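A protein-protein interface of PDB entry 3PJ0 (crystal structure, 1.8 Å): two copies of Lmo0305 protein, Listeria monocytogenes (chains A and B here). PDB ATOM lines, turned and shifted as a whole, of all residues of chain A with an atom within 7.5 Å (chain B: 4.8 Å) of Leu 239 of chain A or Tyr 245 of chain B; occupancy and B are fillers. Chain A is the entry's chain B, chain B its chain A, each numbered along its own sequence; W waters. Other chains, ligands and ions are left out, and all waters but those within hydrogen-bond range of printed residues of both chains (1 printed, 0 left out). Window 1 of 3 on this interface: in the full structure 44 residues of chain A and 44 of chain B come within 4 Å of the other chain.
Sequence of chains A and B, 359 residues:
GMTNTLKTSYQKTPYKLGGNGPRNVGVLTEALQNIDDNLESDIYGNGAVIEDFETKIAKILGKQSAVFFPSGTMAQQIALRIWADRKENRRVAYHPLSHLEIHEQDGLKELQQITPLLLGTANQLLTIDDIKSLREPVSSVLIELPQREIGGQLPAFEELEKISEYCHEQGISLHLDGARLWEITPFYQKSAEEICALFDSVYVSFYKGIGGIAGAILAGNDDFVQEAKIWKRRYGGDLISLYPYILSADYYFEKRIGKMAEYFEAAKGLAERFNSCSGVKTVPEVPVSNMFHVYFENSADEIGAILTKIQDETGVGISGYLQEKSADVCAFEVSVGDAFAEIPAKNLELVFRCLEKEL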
ATOM      1  N   LEU A  28      38.658  -6.840  25.936  1.00  0.00           N
ATOM      2  CA  LEU A  28      37.715  -7.407  24.982  1.00  0.00           C
ATOM      3  C   LEU A  28      37.648  -6.565  23.719  1.00  0.00           C
ATOM      4  O   LEU A  28      37.653  -7.113  22.606  1.00  0.00           O
ATOM      5  CB  LEU A  28      36.327  -7.537  25.614  1.00  0.00           C
ATOM      6  CG  LEU A  28      35.182  -8.127  24.779  1.00  0.00           C
ATOM      7  CD1 LEU A  28      35.477  -9.540  24.213  1.00  0.00           C
ATOM      8  CD2 LEU A  28      33.925  -8.182  25.610  1.00  0.00           C
ATOM      9  N   SER A  41      27.941 -16.522  15.498  1.00  0.00           N
ATOM     10  CA  SER A  41      28.187 -17.083  16.793  1.00  0.00           C
ATOM     11  C   SER A  41      28.264 -18.609  16.695  1.00  0.00           C
ATOM     12  O   SER A  41      27.663 -19.228  15.801  1.00  0.00           O
ATOM     13  CB  SER A  41      27.065 -16.686  17.751  1.00  0.00           C
ATOM     14  OG  SER A  41      27.152 -17.361  18.988  1.00  0.00           O
ATOM     15  N   ASP A  42      29.047 -19.189  17.603  1.00  0.00           N
ATOM     16  CA  ASP A  42      28.993 -20.614  17.837  1.00  0.00           C
ATOM     17  C   ASP A  42      27.574 -20.902  18.365  1.00  0.00           C
ATOM     18  O   ASP A  42      26.910 -19.987  18.866  1.00  0.00           O
ATOM     19  CB  ASP A  42      30.084 -21.069  18.811  1.00  0.00           C
ATOM     20  CG  ASP A  42      30.118 -20.245  20.092  1.00  0.00           C
ATOM     21  OD1 ASP A  42      30.209 -19.001  20.015  1.00  0.00           O
ATOM     22  OD2 ASP A  42      30.079 -20.858  21.164  1.00  0.00           O
ATOM     23  N   ILE A  43      27.097 -22.147  18.238  1.00  0.00           N
ATOM     24  CA  ILE A  43      25.787 -22.546  18.747  1.00  0.00           C
ATOM     25  C   ILE A  43      25.899 -23.868  19.549  1.00  0.00           C
ATOM     26  O   ILE A  43      26.122 -24.957  18.990  1.00  0.00           O
ATOM     27  CB  ILE A  43      24.710 -22.634  17.617  1.00  0.00           C
ATOM     28  CG1 ILE A  43      24.528 -21.279  16.897  1.00  0.00           C
ATOM     29  CG2 ILE A  43      23.352 -23.097  18.175  1.00  0.00           C
ATOM     30  CD1 ILE A  43      23.780 -20.189  17.744  1.00  0.00           C
ATOM     31  N   TYR A  44      25.784 -23.752  20.872  1.00  0.00           N
ATOM     32  CA  TYR A  44      25.877 -24.900  21.798  1.00  0.00           C
ATOM     33  C   TYR A  44      27.001 -25.902  21.412  1.00  0.00           C
ATOM     34  O   TYR A  44      26.750 -27.072  21.101  1.00  0.00           O
ATOM     35  CB  TYR A  44      24.521 -25.599  21.931  1.00  0.00           C
ATOM     36  CG  TYR A  44      23.351 -24.748  22.400  1.00  0.00           C
ATOM     37  CD1 TYR A  44      23.260 -24.333  23.701  1.00  0.00           C
ATOM     38  CD2 TYR A  44      22.314 -24.409  21.544  1.00  0.00           C
ATOM     39  CE1 TYR A  44      22.202 -23.550  24.143  1.00  0.00           C
ATOM     40  CE2 TYR A  44      21.280 -23.604  21.948  1.00  0.00           C
ATOM     41  CZ  TYR A  44      21.176 -23.214  23.290  1.00  0.00           C
ATOM     42  OH  TYR A  44      20.079 -22.491  23.694  1.00  0.00           O
ATOM     43  N   GLY A  45      28.219 -25.382  21.343  1.00  0.00           N
ATOM     44  CA  GLY A  45      29.432 -26.165  21.079  1.00  0.00           C
ATOM     45  C   GLY A  45      29.801 -26.459  19.634  1.00  0.00           C
ATOM     46  O   GLY A  45      30.807 -27.105  19.416  1.00  0.00           O
ATOM     47  N   ASN A  46      28.998 -25.986  18.678  1.00  0.00           N
ATOM     48  CA  ASN A  46      29.243 -26.169  17.246  1.00  0.00           C
ATOM     49  C   ASN A  46      29.399 -24.838  16.541  1.00  0.00           C
ATOM     50  O   ASN A  46      28.967 -23.791  17.051  1.00  0.00           O
ATOM     51  CB  ASN A  46      28.101 -26.952  16.604  1.00  0.00           C
ATOM     52  CG  ASN A  46      27.921 -28.326  17.227  1.00  0.00           C
ATOM     53  OD1 ASN A  46      28.866 -29.091  17.335  1.00  0.00           O
ATOM     54  ND2 ASN A  46      26.714 -28.620  17.665  1.00  0.00           N
ATOM     55  N   ILE A  50      34.115 -21.890  17.292  1.00  0.00           N
ATOM     56  CA  ILE A  50      34.524 -22.783  18.392  1.00  0.00           C
ATOM     57  C   ILE A  50      35.315 -23.994  17.893  1.00  0.00           C
ATOM     58  O   ILE A  50      36.392 -24.338  18.443  1.00  0.00           O
ATOM     59  CB  ILE A  50      33.313 -23.207  19.302  1.00  0.00           C
ATOM     60  CG1 ILE A  50      33.827 -24.023  20.510  1.00  0.00           C
ATOM     61  CG2 ILE A  50      32.259 -23.973  18.500  1.00  0.00           C
ATOM     62  CD1 ILE A  50      32.828 -24.130  21.677  1.00  0.00           C
ATOM     63  N   PHE A  68      36.334 -26.692  24.260  1.00  0.00           N
ATOM     64  CA  PHE A  68      36.469 -25.414  24.953  1.00  0.00           C
ATOM     65  C   PHE A  68      35.451 -25.366  26.109  1.00  0.00           C
ATOM     66  O   PHE A  68      34.235 -25.551  25.893  1.00  0.00           O
ATOM     67  CB  PHE A  68      36.213 -24.260  24.001  1.00  0.00           C
ATOM     68  CG  PHE A  68      36.504 -22.913  24.598  1.00  0.00           C
ATOM     69  CD1 PHE A  68      37.790 -22.405  24.555  1.00  0.00           C
ATOM     70  CD2 PHE A  68      35.521 -22.174  25.207  1.00  0.00           C
ATOM     71  CE1 PHE A  68      38.095 -21.174  25.114  1.00  0.00           C
ATOM     72  CE2 PHE A  68      35.813 -20.912  25.787  1.00  0.00           C
ATOM     73  CZ  PHE A  68      37.102 -20.422  25.734  1.00  0.00           C
ATOM     74  N   PRO A  70      34.027 -23.175  29.695  1.00  0.00           N
ATOM     75  CA  PRO A  70      34.077 -21.837  30.282  1.00  0.00           C
ATOM     76  C   PRO A  70      35.090 -21.759  31.449  1.00  0.00           C
ATOM     77  O   PRO A  70      35.592 -20.670  31.720  1.00  0.00           O
ATOM     78  CB  PRO A  70      32.646 -21.604  30.760  1.00  0.00           C
ATOM     79  CG  PRO A  70      32.064 -22.946  30.914  1.00  0.00           C
ATOM     80  CD  PRO A  70      32.733 -23.839  29.917  1.00  0.00           C
ATOM     81  N   MET A  74      35.394 -26.626  36.005  1.00  0.00           N
ATOM     82  CA  MET A  74      34.439 -27.569  35.414  1.00  0.00           C
ATOM     83  C   MET A  74      35.207 -28.660  34.633  1.00  0.00           C
ATOM     84  O   MET A  74      34.985 -29.871  34.822  1.00  0.00           O
ATOM     85  CB  MET A  74      33.492 -26.795  34.459  1.00  0.00           C
ATOM     86  CG  MET A  74      32.402 -27.631  33.869  1.00  0.00           C
ATOM     87  SD  MET A  74      31.467 -26.537  32.602  1.00  0.00           S
ATOM     88  CE  MET A  74      30.642 -25.143  33.779  1.00  0.00           C
ATOM     89  N   LYS A 232      29.675 -31.547  30.114  1.00  0.00           N
ATOM     90  CA  LYS A 232      29.654 -30.095  29.952  1.00  0.00           C
ATOM     91  C   LYS A 232      28.238 -29.569  29.975  1.00  0.00           C
ATOM     92  O   LYS A 232      27.954 -28.575  30.655  1.00  0.00           O
ATOM     93  CB  LYS A 232      30.355 -29.674  28.653  1.00  0.00           C
ATOM     94  CG  LYS A 232      30.371 -28.178  28.378  1.00  0.00           C
ATOM     95  CD  LYS A 232      31.212 -27.918  27.097  1.00  0.00           C
ATOM     96  CE  LYS A 232      31.169 -26.518  26.610  1.00  0.00           C
ATOM     97  NZ  LYS A 232      31.721 -26.469  25.172  1.00  0.00           N
ATOM     98  N   ARG A 233      27.354 -30.245  29.245  1.00  0.00           N
ATOM     99  CA  ARG A 233      25.943 -29.870  29.245  1.00  0.00           C
ATOM    100  C   ARG A 233      25.312 -30.092  30.614  1.00  0.00           C
ATOM    101  O   ARG A 233      24.518 -29.256  31.078  1.00  0.00           O
ATOM    102  CB  ARG A 233      25.158 -30.579  28.133  1.00  0.00           C
ATOM    103  CG  ARG A 233      23.610 -30.383  28.242  1.00  0.00           C
ATOM    104  CD  ARG A 233      22.933 -30.170  26.903  1.00  0.00           C
ATOM    105  NE  ARG A 233      23.214 -28.818  26.449  1.00  0.00           N
ATOM    106  CZ  ARG A 233      22.559 -27.716  26.827  1.00  0.00           C
ATOM    107  NH1 ARG A 233      21.530 -27.772  27.666  1.00  0.00           N
ATOM    108  NH2 ARG A 233      22.946 -26.536  26.363  1.00  0.00           N
ATOM    109  N   GLY A 236      25.999 -27.271  33.014  1.00  0.00           N
ATOM    110  CA  GLY A 236      25.551 -25.946  32.625  1.00  0.00           C
ATOM    111  C   GLY A 236      26.696 -25.143  31.982  1.00  0.00           C
ATOM    112  O   GLY A 236      26.707 -23.923  32.034  1.00  0.00           O
ATOM    113  N   GLY A 237      27.638 -25.826  31.348  1.00  0.00           N
ATOM    114  CA  GLY A 237      28.766 -25.179  30.652  1.00  0.00           C
ATOM    115  C   GLY A 237      28.611 -25.070  29.141  1.00  0.00           C
ATOM    116  O   GLY A 237      29.412 -24.432  28.498  1.00  0.00           O
ATOM    117  N   ASP A 238      27.589 -25.729  28.585  1.00  0.00           N
ATOM    118  CA  ASP A 238      27.319 -25.720  27.134  1.00  0.00           C
ATOM    119  C   ASP A 238      26.476 -24.487  26.797  1.00  0.00           C
ATOM    120  O   ASP A 238      25.286 -24.560  26.439  1.00  0.00           O
ATOM    121  CB  ASP A 238      26.657 -27.028  26.721  1.00  0.00           C
ATOM    122  CG  ASP A 238      26.421 -27.135  25.212  1.00  0.00           C
ATOM    123  OD1 ASP A 238      27.308 -26.713  24.448  1.00  0.00           O
ATOM    124  OD2 ASP A 238      25.357 -27.657  24.807  1.00  0.00           O
ATOM    125  N   LEU A 239      27.115 -23.333  26.940  1.00  0.00           N
ATOM    126  CA  LEU A 239      26.416 -22.056  26.690  1.00  0.00           C
ATOM    127  C   LEU A 239      26.126 -21.949  25.218  1.00  0.00           C
ATOM    128  O   LEU A 239      26.892 -22.474  24.389  1.00  0.00           O
ATOM    129  CB  LEU A 239      27.307 -20.878  27.141  1.00  0.00           C
ATOM    130  CG  LEU A 239      27.867 -20.929  28.567  1.00  0.00           C
ATOM    131  CD1 LEU A 239      28.552 -19.613  28.961  1.00  0.00           C
ATOM    132  CD2 LEU A 239      26.733 -21.242  29.526  1.00  0.00           C
ATOM    133  N   ILE A 240      25.026 -21.287  24.874  1.00  0.00           N
ATOM    134  CA  ILE A 240      24.690 -21.124  23.462  1.00  0.00           C
ATOM    135  C   ILE A 240      25.883 -20.471  22.719  1.00  0.00           C
ATOM    136  O   ILE A 240      26.264 -20.946  21.667  1.00  0.00           O
ATOM    137  CB  ILE A 240      23.375 -20.326  23.246  1.00  0.00           C
ATOM    138  CG1 ILE A 240      23.033 -20.244  21.750  1.00  0.00           C
ATOM    139  CG2 ILE A 240      23.491 -18.916  23.848  1.00  0.00           C
ATOM    140  CD1 ILE A 240      21.704 -19.611  21.423  1.00  0.00           C
ATOM    141  N   SER A 241      26.471 -19.431  23.310  1.00  0.00           N
ATOM    142  CA  SER A 241      27.529 -18.652  22.677  1.00  0.00           C
ATOM    143  C   SER A 241      28.705 -18.461  23.608  1.00  0.00           C
ATOM    144  O   SER A 241      28.580 -17.773  24.640  1.00  0.00           O
ATOM    145  CB  SER A 241      27.003 -17.258  22.269  1.00  0.00           C
ATOM    146  OG  SER A 241      25.962 -17.330  21.297  1.00  0.00           O
ATOM    147  N   LEU A 242      29.836 -19.067  23.249  1.00  0.00           N
ATOM    148  CA  LEU A 242      31.085 -18.923  24.000  1.00  0.00           C
ATOM    149  C   LEU A 242      32.067 -18.008  23.252  1.00  0.00           C
ATOM    150  O   LEU A 242      33.162 -17.734  23.759  1.00  0.00           O
ATOM    151  CB  LEU A 242      31.713 -20.288  24.287  1.00  0.00           C
ATOM    152  CG  LEU A 242      30.995 -21.120  25.346  1.00  0.00           C
ATOM    153  CD1 LEU A 242      31.446 -22.595  25.396  1.00  0.00           C
ATOM    154  CD2 LEU A 242      31.183 -20.404  26.700  1.00  0.00           C
ATOM    155  N   TYR A 243      31.673 -17.487  22.087  1.00  0.00           N
ATOM    156  CA  TYR A 243      32.617 -16.691  21.284  1.00  0.00           C
ATOM    157  C   TYR A 243      33.316 -15.519  22.009  1.00  0.00           C
ATOM    158  O   TYR A 243      34.462 -15.256  21.715  1.00  0.00           O
ATOM    159  CB  TYR A 243      32.025 -16.231  19.924  1.00  0.00           C
ATOM    160  CG  TYR A 243      30.966 -15.166  20.034  1.00  0.00           C
ATOM    161  CD1 TYR A 243      31.314 -13.814  20.168  1.00  0.00           C
ATOM    162  CD2 TYR A 243      29.618 -15.499  20.025  1.00  0.00           C
ATOM    163  CE1 TYR A 243      30.345 -12.846  20.265  1.00  0.00           C
ATOM    164  CE2 TYR A 243      28.645 -14.530  20.123  1.00  0.00           C
ATOM    165  CZ  TYR A 243      29.022 -13.200  20.260  1.00  0.00           C
ATOM    166  OH  TYR A 243      28.060 -12.230  20.321  1.00  0.00           O
ATOM    167  N   PRO A 244      32.644 -14.818  22.946  1.00  0.00           N
ATOM    168  CA  PRO A 244      33.350 -13.720  23.630  1.00  0.00           C
ATOM    169  C   PRO A 244      34.655 -14.166  24.289  1.00  0.00           C
ATOM    170  O   PRO A 244      35.643 -13.424  24.266  1.00  0.00           O
ATOM    171  CB  PRO A 244      32.326 -13.256  24.668  1.00  0.00           C
ATOM    172  CG  PRO A 244      31.021 -13.628  24.083  1.00  0.00           C
ATOM    173  CD  PRO A 244      31.260 -14.939  23.446  1.00  0.00           C
ATOM    174  N   TYR A 245      34.650 -15.383  24.836  1.00  0.00           N
ATOM    175  CA  TYR A 245      35.832 -15.975  25.463  1.00  0.00           C
ATOM    176  C   TYR A 245      36.748 -16.656  24.459  1.00  0.00           C
ATOM    177  O   TYR A 245      37.975 -16.631  24.600  1.00  0.00           O
ATOM    178  CB  TYR A 245      35.452 -16.985  26.556  1.00  0.00           C
ATOM    179  CG  TYR A 245      34.679 -16.421  27.729  1.00  0.00           C
ATOM    180  CD1 TYR A 245      35.029 -15.218  28.310  1.00  0.00           C
ATOM    181  CD2 TYR A 245      33.645 -17.151  28.313  1.00  0.00           C
ATOM    182  CE1 TYR A 245      34.339 -14.718  29.420  1.00  0.00           C
ATOM    183  CE2 TYR A 245      32.951 -16.667  29.428  1.00  0.00           C
ATOM    184  CZ  TYR A 245      33.296 -15.452  29.971  1.00  0.00           C
ATOM    185  OH  TYR A 245      32.600 -14.975  31.063  1.00  0.00           O
ATOM    186  N   ILE A 246      36.177 -17.298  23.459  1.00  0.00           N
ATOM    187  CA  ILE A 246      37.000 -17.935  22.430  1.00  0.00           C
ATOM    188  C   ILE A 246      37.827 -16.926  21.608  1.00  0.00           C
ATOM    189  O   ILE A 246      39.028 -17.087  21.410  1.00  0.00           O
ATOM    190  CB  ILE A 246      36.158 -18.759  21.453  1.00  0.00           C
ATOM    191  CG1 ILE A 246      35.363 -19.823  22.214  1.00  0.00           C
ATOM    192  CG2 ILE A 246      37.077 -19.378  20.388  1.00  0.00           C
ATOM    193  CD1 ILE A 246      34.161 -20.444  21.465  1.00  0.00           C
ATOM    194  N   PHE B  68      24.354 -13.655  39.381  1.00  0.00           N
ATOM    195  CA  PHE B  68      24.472 -13.826  37.952  1.00  0.00           C
ATOM    196  C   PHE B  68      25.196 -15.139  37.626  1.00  0.00           C
ATOM    197  O   PHE B  68      26.341 -15.372  38.065  1.00  0.00           O
ATOM    198  CB  PHE B  68      25.173 -12.625  37.293  1.00  0.00           C
ATOM    199  CG  PHE B  68      25.153 -12.688  35.790  1.00  0.00           C
ATOM    200  CD1 PHE B  68      24.097 -12.153  35.091  1.00  0.00           C
ATOM    201  CD2 PHE B  68      26.178 -13.321  35.083  1.00  0.00           C
ATOM    202  CE1 PHE B  68      24.053 -12.209  33.697  1.00  0.00           C
ATOM    203  CE2 PHE B  68      26.144 -13.405  33.701  1.00  0.00           C
ATOM    204  CZ  PHE B  68      25.069 -12.854  32.997  1.00  0.00           C
ATOM    205  N   PRO B  70      26.371 -18.135  34.501  1.00  0.00           N
ATOM    206  CA  PRO B  70      26.582 -18.292  33.061  1.00  0.00           C
ATOM    207  C   PRO B  70      25.396 -18.965  32.360  1.00  0.00           C
ATOM    208  O   PRO B  70      25.166 -18.724  31.175  1.00  0.00           O
ATOM    209  CB  PRO B  70      27.830 -19.172  32.978  1.00  0.00           C
ATOM    210  CG  PRO B  70      27.993 -19.791  34.349  1.00  0.00           C
ATOM    211  CD  PRO B  70      27.413 -18.826  35.296  1.00  0.00           C
ATOM    212  N   SER B  71      24.664 -19.817  33.071  1.00  0.00           N
ATOM    213  CA  SER B  71      23.532 -20.520  32.491  1.00  0.00           C
ATOM    214  C   SER B  71      22.436 -20.855  33.485  1.00  0.00           C
ATOM    215  O   SER B  71      22.671 -20.989  34.706  1.00  0.00           O
ATOM    216  CB  SER B  71      24.022 -21.843  31.878  1.00  0.00           C
ATOM    217  OG  SER B  71      24.354 -22.758  32.890  1.00  0.00           O
ATOM    218  N   ILE B 213      23.067 -12.401  24.579  1.00  0.00           N
ATOM    219  CA  ILE B 213      24.012 -13.410  24.112  1.00  0.00           C
ATOM    220  C   ILE B 213      23.824 -14.703  24.911  1.00  0.00           C
ATOM    221  O   ILE B 213      23.580 -15.755  24.326  1.00  0.00           O
ATOM    222  CB  ILE B 213      25.473 -12.881  24.188  1.00  0.00           C
ATOM    223  CG1 ILE B 213      25.606 -11.611  23.310  1.00  0.00           C
ATOM    224  CG2 ILE B 213      26.472 -13.977  23.744  1.00  0.00           C
ATOM    225  CD1 ILE B 213      26.991 -10.919  23.318  1.00  0.00           C
ATOM    226  N   ALA B 214      23.979 -14.597  26.239  1.00  0.00           N
ATOM    227  CA  ALA B 214      23.814 -15.718  27.158  1.00  0.00           C
ATOM    228  C   ALA B 214      23.744 -15.196  28.587  1.00  0.00           C
ATOM    229  O   ALA B 214      23.983 -14.018  28.840  1.00  0.00           O
ATOM    230  CB  ALA B 214      24.960 -16.720  27.023  1.00  0.00           C
ATOM    231  N   LEU B 242      32.788 -12.333  34.135  1.00  0.00           N
ATOM    232  CA  LEU B 242      31.501 -12.574  33.446  1.00  0.00           C
ATOM    233  C   LEU B 242      30.989 -11.319  32.721  1.00  0.00           C
ATOM    234  O   LEU B 242      29.937 -11.367  32.059  1.00  0.00           O
ATOM    235  CB  LEU B 242      30.447 -13.074  34.453  1.00  0.00           C
ATOM    236  CG  LEU B 242      30.673 -14.518  34.908  1.00  0.00           C
ATOM    237  CD1 LEU B 242      29.843 -14.854  36.166  1.00  0.00           C
ATOM    238  CD2 LEU B 242      30.383 -15.545  33.778  1.00  0.00           C
ATOM    239  N   TYR B 243      31.729 -10.210  32.777  1.00  0.00           N
ATOM    240  CA  TYR B 243      31.222  -8.976  32.155  1.00  0.00           C
ATOM    241  C   TYR B 243      30.784  -9.067  30.663  1.00  0.00           C
ATOM    242  O   TYR B 243      29.854  -8.347  30.297  1.00  0.00           O
ATOM    243  CB  TYR B 243      32.173  -7.778  32.346  1.00  0.00           C
ATOM    244  CG  TYR B 243      33.427  -7.836  31.529  1.00  0.00           C
ATOM    245  CD1 TYR B 243      33.437  -7.400  30.203  1.00  0.00           C
ATOM    246  CD2 TYR B 243      34.620  -8.315  32.070  1.00  0.00           C
ATOM    247  CE1 TYR B 243      34.613  -7.464  29.447  1.00  0.00           C
ATOM    248  CE2 TYR B 243      35.780  -8.359  31.323  1.00  0.00           C
ATOM    249  CZ  TYR B 243      35.775  -7.941  30.023  1.00  0.00           C
ATOM    250  OH  TYR B 243      36.919  -7.985  29.269  1.00  0.00           O
ATOM    251  N   PRO B 244      31.425  -9.924  29.825  1.00  0.00           N
ATOM    252  CA  PRO B 244      30.906  -9.930  28.454  1.00  0.00           C
ATOM    253  C   PRO B 244      29.418 -10.268  28.355  1.00  0.00           C
ATOM    254  O   PRO B 244      28.697  -9.688  27.514  1.00  0.00           O
ATOM    255  CB  PRO B 244      31.795 -10.967  27.733  1.00  0.00           C
ATOM    256  CG  PRO B 244      33.087 -10.970  28.515  1.00  0.00           C
ATOM    257  CD  PRO B 244      32.645 -10.732  29.951  1.00  0.00           C
ATOM    258  N   TYR B 245      28.969 -11.180  29.208  1.00  0.00           N
ATOM    259  CA  TYR B 245      27.569 -11.582  29.261  1.00  0.00           C
ATOM    260  C   TYR B 245      26.761 -10.610  30.118  1.00  0.00           C
ATOM    261  O   TYR B 245      25.631 -10.339  29.814  1.00  0.00           O
ATOM    262  CB  TYR B 245      27.399 -13.017  29.795  1.00  0.00           C
ATOM    263  CG  TYR B 245      28.073 -14.091  28.987  1.00  0.00           C
ATOM    264  CD1 TYR B 245      28.007 -14.100  27.600  1.00  0.00           C
ATOM    265  CD2 TYR B 245      28.745 -15.125  29.610  1.00  0.00           C
ATOM    266  CE1 TYR B 245      28.637 -15.102  26.855  1.00  0.00           C
ATOM    267  CE2 TYR B 245      29.365 -16.139  28.874  1.00  0.00           C
ATOM    268  CZ  TYR B 245      29.302 -16.117  27.502  1.00  0.00           C
ATOM    269  OH  TYR B 245      29.922 -17.115  26.786  1.00  0.00           O
ATOM    270  N   ILE B 246      27.343 -10.058  31.186  1.00  0.00           N
ATOM    271  CA  ILE B 246      26.578  -9.094  32.030  1.00  0.00           C
ATOM    272  C   ILE B 246      26.263  -7.811  31.257  1.00  0.00           C
ATOM    273  O   ILE B 246      25.105  -7.365  31.186  1.00  0.00           O
ATOM    274  CB  ILE B 246      27.333  -8.717  33.336  1.00  0.00           C
ATOM    275  CG1 ILE B 246      27.486  -9.942  34.241  1.00  0.00           C
ATOM    276  CG2 ILE B 246      26.591  -7.607  34.135  1.00  0.00           C
ATOM    277  CD1 ILE B 246      28.615  -9.758  35.250  1.00  0.00           C
ATOM    278  N   LEU B 247      27.287  -7.229  30.644  1.00  0.00           N
ATOM    279  CA  LEU B 247      27.063  -6.001  29.846  1.00  0.00           C
ATOM    280  C   LEU B 247      26.036  -6.183  28.715  1.00  0.00           C
ATOM    281  O   LEU B 247      25.183  -5.292  28.499  1.00  0.00           O
ATOM    282  CB  LEU B 247      28.366  -5.421  29.327  1.00  0.00           C
ATOM    283  CG  LEU B 247      29.338  -4.943  30.429  1.00  0.00           C
ATOM    284  CD1 LEU B 247      30.706  -4.644  29.822  1.00  0.00           C
ATOM    285  CD2 LEU B 247      28.798  -3.744  31.308  1.00  0.00           C
ATOM    286  N   SER B 248      26.164  -7.278  27.952  1.00  0.00           N
ATOM    287  CA  SER B 248      25.221  -7.571  26.882  1.00  0.00           C
ATOM    288  C   SER B 248      23.825  -7.871  27.435  1.00  0.00           C
ATOM    289  O   SER B 248      22.832  -7.443  26.827  1.00  0.00           O
ATOM    290  CB  SER B 248      25.708  -8.704  25.967  1.00  0.00           C
ATOM    291  OG  SER B 248      26.078  -9.834  26.717  1.00  0.00           O
ATOM    292  N   ALA B 249      23.741  -8.576  28.568  1.00  0.00           N
ATOM    293  CA  ALA B 249      22.422  -8.863  29.196  1.00  0.00           C
ATOM    294  C   ALA B 249      21.736  -7.571  29.580  1.00  0.00           C
ATOM    295  O   ALA B 249      20.593  -7.350  29.237  1.00  0.00           O
ATOM    296  CB  ALA B 249      22.563  -9.769  30.451  1.00  0.00           C
HETATM  297  O   HOH W   1      23.470 -15.949  21.668  1.00  0.00           O
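The side-chain hydroxyl (OG) of Ser 71 of chain B is in hydrogen-bond range of the backbone carbonyl oxygen (O) of Gly 236 of chain A.
The side-chain hydroxyl of Tyr 245 of chain B is in hydrogen-bond range of the backbone carbonyl oxygen of Ser 241 of chain A (2.6 Å).
The side-chain hydroxyl (OG) of Ser 241 of chain A lies within hydrogen-bond range of the side-chain hydroxyl (OG) of Ser 41 of chain A.
The backbone NH of Tyr 243 of chain A sits at hydrogen-bond distance from the side-chain carboxylate of Asp 42 of chain A (3.0 Å).
N of Leu 242 of chain A is in hydrogen-bond range of OD2 of Asp 42 of chain A (2.8 Å).
The side-chain hydroxyl of Ser 248 of chain B is in hydrogen-bond range of the backbone carbonyl oxygen of Tyr 245 of chain B (3.2 Å).
CB of Leu 28 of chain A touches OH of Tyr 243 of chain B (3.7 Å).
CD2 of Leu 239 of chain A touches O of Pro 70 of chain B (3.4 Å).
CB of Ser 71 of chain B touches CD2 of Leu 239 of chain A, at 3.6 Å.
CG2 of Ile 240 of chain A touches O of Ile 213 of chain B (3.2 Å).
Ser 241 of chain A touches Ile 213 of chain B.
OH of Tyr 245 of chain B touches CA of Leu 242 of chain A (3.5 Å).
Tyr 243 of chain A touches Ile 213 of chain B.
CB of Pro 244 of chain B touches CB of Pro 244 of chain A, 3.9 Å away.
Leu 242 of chain B touches Tyr 245 of chain A (CD2 to OH, 3.6 Å).
Tyr 245 of chain A touches Tyr 245 of chain B.
Of the printed residues of chain A, Tyr 245 of chain B touches Leu 239 (3.6 Å), Ser 241 (2.6 Å), Leu 242 (3.5 Å), Pro 244 (3.9 Å) and Tyr 245 (3.7 Å).
Printed residues of chain B within 4 Å of Tyr 243 of chain A: Ile 213.
Of the printed residues of chain A, Leu 242 of chain B touches Tyr 245.
Of the printed residues of chain A, Ser 71 of chain B touches Gly 236 and Leu 239.
Of the printed residues of chain B, Pro 244 of chain A touches Pro 244 (3.9 Å) and Tyr 245 (3.9 Å).
Phe 68 of chain A touches none of the printed residues of chain B.
The nearest printed residue of chain B that does not touch Leu 239 of chain A is Ala 214 of chain B (4.8 Å).
Printed residues of chain B that touch a printed residue of chain A: Pro 70, Ser 71, Ile 213, Leu 242, Tyr 243, Pro 244 and Tyr 245.
Hydrophobic or aromatic side chains of chain B that line the printed part of chain A: Ile 213, Leu 242, Tyr 243, Pro 244 and Tyr 245.
Of the 24 printed residues of chain A, 9 touch a printed residue of chain B.
Among the printed residues, no Asp or Glu carboxylate lies within 4 Å of a Lys or Arg side-chain nitrogen of the other chain.
Leu 242 of chain A touches Tyr 245 of chain B, and with the chains exchanged Tyr 245 of chain A touches Leu 242 of chain B.
Pro 244 of chain B touches its own counterpart, Pro 244 of chain A.
Pro 244 of chain A touches Tyr 245 of chain B, but with the chains exchanged Tyr 245 of chain A does not touch Pro 244 of chain B (4.1 Å).
Tyr 245 of chain B touches its own counterpart, Tyr 245 of chain A.
Of the 14 pairs that touch across the chains among the printed residues, 4 have their exchanged pair printed and touching as well.
Water W1 bridges the backbone carbonyl oxygen of Ile 213 of chain B and the side-chain hydroxyl of Ser 241 of chain A.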
